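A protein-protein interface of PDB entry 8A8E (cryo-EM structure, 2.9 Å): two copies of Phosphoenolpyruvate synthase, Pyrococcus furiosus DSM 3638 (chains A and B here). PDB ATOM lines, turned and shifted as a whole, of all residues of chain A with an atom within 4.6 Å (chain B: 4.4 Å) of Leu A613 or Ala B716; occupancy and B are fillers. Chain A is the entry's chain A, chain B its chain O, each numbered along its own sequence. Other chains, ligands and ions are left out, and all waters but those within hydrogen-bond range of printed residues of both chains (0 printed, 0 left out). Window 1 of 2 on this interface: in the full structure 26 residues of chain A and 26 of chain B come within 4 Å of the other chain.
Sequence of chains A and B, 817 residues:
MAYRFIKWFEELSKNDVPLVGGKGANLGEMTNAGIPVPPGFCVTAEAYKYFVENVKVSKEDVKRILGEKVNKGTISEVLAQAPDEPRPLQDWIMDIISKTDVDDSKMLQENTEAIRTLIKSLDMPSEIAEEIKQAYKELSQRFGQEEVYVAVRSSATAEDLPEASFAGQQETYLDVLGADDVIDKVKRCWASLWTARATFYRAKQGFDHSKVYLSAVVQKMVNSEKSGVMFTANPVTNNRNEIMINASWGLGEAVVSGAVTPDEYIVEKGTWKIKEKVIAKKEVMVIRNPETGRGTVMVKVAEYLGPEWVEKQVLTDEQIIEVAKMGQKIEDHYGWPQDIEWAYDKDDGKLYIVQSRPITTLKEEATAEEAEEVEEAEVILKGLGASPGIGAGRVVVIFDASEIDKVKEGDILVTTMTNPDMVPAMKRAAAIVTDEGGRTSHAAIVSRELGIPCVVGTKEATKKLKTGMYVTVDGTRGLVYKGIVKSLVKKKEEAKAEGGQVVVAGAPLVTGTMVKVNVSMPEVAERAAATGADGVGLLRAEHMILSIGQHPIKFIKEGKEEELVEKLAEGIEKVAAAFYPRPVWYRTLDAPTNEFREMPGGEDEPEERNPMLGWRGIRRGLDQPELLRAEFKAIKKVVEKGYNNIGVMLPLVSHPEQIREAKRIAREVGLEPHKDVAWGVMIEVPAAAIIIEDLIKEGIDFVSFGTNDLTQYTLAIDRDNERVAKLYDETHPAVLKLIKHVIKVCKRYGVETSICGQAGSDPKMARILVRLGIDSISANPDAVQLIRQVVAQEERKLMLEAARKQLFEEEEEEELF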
ATOM      1  N   ASN A 610       3.032   7.976 -12.469  1.00  0.00           N
ATOM      2  CA  ASN A 610       4.348   8.100 -13.097  1.00  0.00           C
ATOM      3  C   ASN A 610       4.250   8.506 -14.569  1.00  0.00           C
ATOM      4  O   ASN A 610       4.315   7.651 -15.448  1.00  0.00           O
ATOM      5  CB  ASN A 610       5.114   6.785 -12.977  1.00  0.00           C
ATOM      6  CG  ASN A 610       5.266   6.329 -11.543  1.00  0.00           C
ATOM      7  OD1 ASN A 610       6.161   6.778 -10.830  1.00  0.00           O
ATOM      8  ND2 ASN A 610       4.390   5.432 -11.111  1.00  0.00           N
ATOM      9  N   PRO A 611       4.114   9.815 -14.848  1.00  0.00           N
ATOM     10  CA  PRO A 611       3.932  10.230 -16.246  1.00  0.00           C
ATOM     11  C   PRO A 611       5.177  10.074 -17.102  1.00  0.00           C
ATOM     12  O   PRO A 611       5.082  10.237 -18.323  1.00  0.00           O
ATOM     13  CB  PRO A 611       3.530  11.709 -16.131  1.00  0.00           C
ATOM     14  CG  PRO A 611       3.409  11.996 -14.662  1.00  0.00           C
ATOM     15  CD  PRO A 611       4.203  10.968 -13.945  1.00  0.00           C
ATOM     16  N   MET A 612       6.336   9.775 -16.507  1.00  0.00           N
ATOM     17  CA  MET A 612       7.543   9.543 -17.292  1.00  0.00           C
ATOM     18  C   MET A 612       7.565   8.160 -17.921  1.00  0.00           C
ATOM     19  O   MET A 612       8.188   7.982 -18.972  1.00  0.00           O
ATOM     20  CB  MET A 612       8.788   9.723 -16.426  1.00  0.00           C
ATOM     21  CG  MET A 612       9.410  11.099 -16.517  1.00  0.00           C
ATOM     22  SD  MET A 612      11.194  11.069 -16.283  1.00  0.00           S
ATOM     23  CE  MET A 612      11.306  11.119 -14.502  1.00  0.00           C
ATOM     24  N   LEU A 613       6.906   7.183 -17.306  1.00  0.00           N
ATOM     25  CA  LEU A 613       6.846   5.818 -17.813  1.00  0.00           C
ATOM     26  C   LEU A 613       5.449   5.481 -18.317  1.00  0.00           C
ATOM     27  O   LEU A 613       4.994   4.343 -18.215  1.00  0.00           O
ATOM     28  CB  LEU A 613       7.278   4.828 -16.739  1.00  0.00           C
ATOM     29  CG  LEU A 613       8.509   5.236 -15.939  1.00  0.00           C
ATOM     30  CD1 LEU A 613       8.439   4.682 -14.543  1.00  0.00           C
ATOM     31  CD2 LEU A 613       9.761   4.759 -16.637  1.00  0.00           C
ATOM     32  N   GLY A 614       4.757   6.468 -18.874  1.00  0.00           N
ATOM     33  CA  GLY A 614       3.366   6.281 -19.221  1.00  0.00           C
ATOM     34  C   GLY A 614       3.028   6.383 -20.692  1.00  0.00           C
ATOM     35  O   GLY A 614       3.815   5.997 -21.558  1.00  0.00           O
ATOM     36  N   ARG A 619       3.848   5.768 -28.780  1.00  0.00           N
ATOM     37  CA  ARG A 619       2.797   4.882 -28.289  1.00  0.00           C
ATOM     38  C   ARG A 619       1.430   5.545 -28.417  1.00  0.00           C
ATOM     39  O   ARG A 619       0.542   5.061 -29.133  1.00  0.00           O
ATOM     40  CB  ARG A 619       3.061   4.501 -26.833  1.00  0.00           C
ATOM     41  CG  ARG A 619       4.444   3.983 -26.539  1.00  0.00           C
ATOM     42  CD  ARG A 619       4.725   4.047 -25.052  1.00  0.00           C
ATOM     43  NE  ARG A 619       6.085   3.635 -24.730  1.00  0.00           N
ATOM     44  CZ  ARG A 619       6.589   3.621 -23.502  1.00  0.00           C
ATOM     45  NH1 ARG A 619       5.847   3.996 -22.474  1.00  0.00           N
ATOM     46  NH2 ARG A 619       7.838   3.230 -23.306  1.00  0.00           N
ATOM     47  N   VAL A 685      15.370   4.889 -24.660  1.00  0.00           N
ATOM     48  CA  VAL A 685      15.176   3.792 -23.718  1.00  0.00           C
ATOM     49  C   VAL A 685      16.367   2.849 -23.839  1.00  0.00           C
ATOM     50  O   VAL A 685      16.893   2.658 -24.943  1.00  0.00           O
ATOM     51  CB  VAL A 685      13.841   3.067 -23.961  1.00  0.00           C
ATOM     52  CG1 VAL A 685      12.703   4.050 -23.931  1.00  0.00           C
ATOM     53  CG2 VAL A 685      13.851   2.338 -25.282  1.00  0.00           C
ATOM     54  N   TYR A 713      16.654   7.138 -17.455  1.00  0.00           N
ATOM     55  CA  TYR A 713      16.123   5.781 -17.407  1.00  0.00           C
ATOM     56  C   TYR A 713      17.178   4.741 -17.076  1.00  0.00           C
ATOM     57  O   TYR A 713      16.826   3.653 -16.615  1.00  0.00           O
ATOM     58  CB  TYR A 713      15.471   5.409 -18.734  1.00  0.00           C
ATOM     59  CG  TYR A 713      14.198   6.150 -19.018  1.00  0.00           C
ATOM     60  CD1 TYR A 713      13.234   6.307 -18.043  1.00  0.00           C
ATOM     61  CD2 TYR A 713      13.963   6.695 -20.264  1.00  0.00           C
ATOM     62  CE1 TYR A 713      12.071   6.989 -18.303  1.00  0.00           C
ATOM     63  CE2 TYR A 713      12.809   7.378 -20.533  1.00  0.00           C
ATOM     64  CZ  TYR A 713      11.865   7.524 -19.551  1.00  0.00           C
ATOM     65  OH  TYR A 713      10.707   8.207 -19.827  1.00  0.00           O
ATOM     66  N   MET B 612       8.577   6.046  -8.339  1.00  0.00           N
ATOM     67  CA  MET B 612       9.391   4.903  -8.736  1.00  0.00           C
ATOM     68  C   MET B 612      10.843   5.284  -8.969  1.00  0.00           C
ATOM     69  O   MET B 612      11.727   4.438  -8.799  1.00  0.00           O
ATOM     70  CB  MET B 612       8.830   4.259 -10.002  1.00  0.00           C
ATOM     71  CG  MET B 612       7.919   3.079  -9.742  1.00  0.00           C
ATOM     72  SD  MET B 612       7.984   1.852 -11.057  1.00  0.00           S
ATOM     73  CE  MET B 612       6.803   2.529 -12.214  1.00  0.00           C
ATOM     74  N   GLN B 712      10.865  -3.335 -15.772  1.00  0.00           N
ATOM     75  CA  GLN B 712      10.169  -2.057 -15.854  1.00  0.00           C
ATOM     76  C   GLN B 712      11.113  -0.911 -16.204  1.00  0.00           C
ATOM     77  O   GLN B 712      10.771  -0.066 -17.034  1.00  0.00           O
ATOM     78  CB  GLN B 712       9.434  -1.777 -14.550  1.00  0.00           C
ATOM     79  CG  GLN B 712       8.033  -2.343 -14.526  1.00  0.00           C
ATOM     80  CD  GLN B 712       7.377  -2.203 -13.182  1.00  0.00           C
ATOM     81  OE1 GLN B 712       7.978  -2.491 -12.152  1.00  0.00           O
ATOM     82  NE2 GLN B 712       6.135  -1.750 -13.179  1.00  0.00           N
ATOM     83  N   TYR B 713      12.299  -0.863 -15.600  1.00  0.00           N
ATOM     84  CA  TYR B 713      13.233   0.220 -15.884  1.00  0.00           C
ATOM     85  C   TYR B 713      13.918   0.078 -17.232  1.00  0.00           C
ATOM     86  O   TYR B 713      14.400   1.077 -17.769  1.00  0.00           O
ATOM     87  CB  TYR B 713      14.303   0.309 -14.801  1.00  0.00           C
ATOM     88  CG  TYR B 713      13.790   0.782 -13.473  1.00  0.00           C
ATOM     89  CD1 TYR B 713      12.935   1.861 -13.385  1.00  0.00           C
ATOM     90  CD2 TYR B 713      14.161   0.143 -12.307  1.00  0.00           C
ATOM     91  CE1 TYR B 713      12.463   2.290 -12.169  1.00  0.00           C
ATOM     92  CE2 TYR B 713      13.695   0.562 -11.090  1.00  0.00           C
ATOM     93  CZ  TYR B 713      12.846   1.635 -11.024  1.00  0.00           C
ATOM     94  OH  TYR B 713      12.385   2.053  -9.802  1.00  0.00           O
ATOM     95  N   THR B 714      13.986  -1.130 -17.786  1.00  0.00           N
ATOM     96  CA  THR B 714      14.671  -1.302 -19.058  1.00  0.00           C
ATOM     97  C   THR B 714      13.794  -0.904 -20.238  1.00  0.00           C
ATOM     98  O   THR B 714      14.296  -0.341 -21.215  1.00  0.00           O
ATOM     99  CB  THR B 714      15.141  -2.750 -19.193  1.00  0.00           C
ATOM    100  OG1 THR B 714      16.064  -3.044 -18.140  1.00  0.00           O
ATOM    101  CG2 THR B 714      15.827  -2.978 -20.520  1.00  0.00           C
ATOM    102  N   LEU B 715      12.493  -1.164 -20.162  1.00  0.00           N
ATOM    103  CA  LEU B 715      11.572  -0.850 -21.242  1.00  0.00           C
ATOM    104  C   LEU B 715      10.891   0.497 -21.067  1.00  0.00           C
ATOM    105  O   LEU B 715      10.091   0.880 -21.923  1.00  0.00           O
ATOM    106  CB  LEU B 715      10.512  -1.945 -21.372  1.00  0.00           C
ATOM    107  CG  LEU B 715      10.968  -3.380 -21.624  1.00  0.00           C
ATOM    108  CD1 LEU B 715       9.792  -4.325 -21.495  1.00  0.00           C
ATOM    109  CD2 LEU B 715      11.609  -3.527 -22.982  1.00  0.00           C
ATOM    110  N   ALA B 716      11.197   1.224 -19.996  1.00  0.00           N
ATOM    111  CA  ALA B 716      10.599   2.528 -19.708  1.00  0.00           C
ATOM    112  C   ALA B 716       9.075   2.446 -19.741  1.00  0.00           C
ATOM    113  O   ALA B 716       8.402   3.079 -20.553  1.00  0.00           O
ATOM    114  CB  ALA B 716      11.115   3.592 -20.679  1.00  0.00           C
ATOM    115  N   ILE B 717       8.535   1.645 -18.830  1.00  0.00           N
ATOM    116  CA  ILE B 717       7.122   1.288 -18.856  1.00  0.00           C
ATOM    117  C   ILE B 717       6.669   0.989 -17.440  1.00  0.00           C
ATOM    118  O   ILE B 717       7.368   0.309 -16.686  1.00  0.00           O
ATOM    119  CB  ILE B 717       6.872   0.089 -19.791  1.00  0.00           C
ATOM    120  CG1 ILE B 717       6.493   0.583 -21.183  1.00  0.00           C
ATOM    121  CG2 ILE B 717       5.823  -0.845 -19.236  1.00  0.00           C
ATOM    122  CD1 ILE B 717       6.292  -0.511 -22.175  1.00  0.00           C
ATOM    123  N   ASP B 718       5.507   1.516 -17.075  1.00  0.00           N
ATOM    124  CA  ASP B 718       4.860   1.180 -15.819  1.00  0.00           C
ATOM    125  C   ASP B 718       3.823   0.091 -16.056  1.00  0.00           C
ATOM    126  O   ASP B 718       3.056   0.147 -17.020  1.00  0.00           O
ATOM    127  CB  ASP B 718       4.199   2.413 -15.208  1.00  0.00           C
ATOM    128  CG  ASP B 718       3.728   2.179 -13.794  1.00  0.00           C
ATOM    129  OD1 ASP B 718       3.982   1.087 -13.255  1.00  0.00           O
ATOM    130  OD2 ASP B 718       3.102   3.089 -13.218  1.00  0.00           O
ATOM    131  N   VAL B 724      -0.413   1.015 -21.184  1.00  0.00           N
ATOM    132  CA  VAL B 724       0.868   0.514 -21.678  1.00  0.00           C
ATOM    133  C   VAL B 724       1.306  -0.787 -21.019  1.00  0.00           C
ATOM    134  O   VAL B 724       2.462  -1.196 -21.206  1.00  0.00           O
ATOM    135  CB  VAL B 724       1.986   1.569 -21.522  1.00  0.00           C
ATOM    136  CG1 VAL B 724       1.687   2.780 -22.379  1.00  0.00           C
ATOM    137  CG2 VAL B 724       2.143   1.974 -20.073  1.00  0.00           C
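The backbone carbonyl oxygen of Gln B712 lies within hydrogen-bond range of the backbone NH of Ile B717, at 3.3 Å.
O of Gly A614 sits at hydrogen-bond distance from NH1 of Arg A619, 3.0 Å away.
The backbone carbonyl oxygen of Met A612 sits at hydrogen-bond distance from the side-chain hydroxyl of Tyr A713, 2.7 Å away.
The backbone carbonyl oxygen of Met B612 sits at hydrogen-bond distance from the side-chain hydroxyl of Tyr B713 (2.7 Å).
Met B612 touches Asn A610 (N to OD1, 3.5 Å).
CE of Met B612 touches CD1 of Leu A613, 3.6 Å away.
Leu A613 touches Ala B716 (CD2 to CA, 3.9 Å).
Leu A613 touches Ile B717.
O of Gly A614 touches CG1 of Val B724, 3.9 Å away.
Arg A619 touches Leu B715 (NH2 to O, 3.5 Å).
NH2 of Arg A619 touches CG1 of Ile B717, at 3.7 Å.
Val A685 touches Ala B716 (CG1 to CB, 3.6 Å).
Tyr B713 touches Tyr A713.
Pro A611 touches none of the printed residues of chain B.
Leu A613 touches just these residues of chain B: Met B612, Ala B716, Ile B717 and Asp B718.
Printed residues of chain B within 4 Å of Gly A614: Val B724 (3.9 Å).
Gln B712 touches none of the printed residues of chain A.
Of the printed residues of chain A, Ala B716 touches Leu A613 (3.9 Å), Arg A619 (2.8 Å) and Val A685 (3.6 Å).
Printed residues of chain A within 4 Å of Val B724: Gly A614 (3.9 Å).
The nearest residue of chain B that does not touch Leu A613 is Val B724 (4.1 Å).
The nearest printed residue of chain A that does not touch Tyr B713 is Leu A613 (5.2 Å).
The backbone carbonyl oxygen (O) of Leu A613 is in hydrogen-bond range of the backbone NH (N) of Asp B718 (3.1 Å).
The side-chain amide nitrogen (ND2) of Asn A610 lies within hydrogen-bond range of the side-chain carboxylate (OD2) of Asp B718 (3.4 Å).
O of Ala B716 lies within hydrogen-bond range of NH2 of Arg A619, 2.8 Å away.
Tyr A713 touches its own counterpart, Tyr B713.
Positions printed for both chains: 612 and 713.
Hydrophobic or aromatic side chains of chain A that line the printed part of chain B: Leu A613 and Val A685.
Among the printed residues, 12 pairs touch across the chains.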
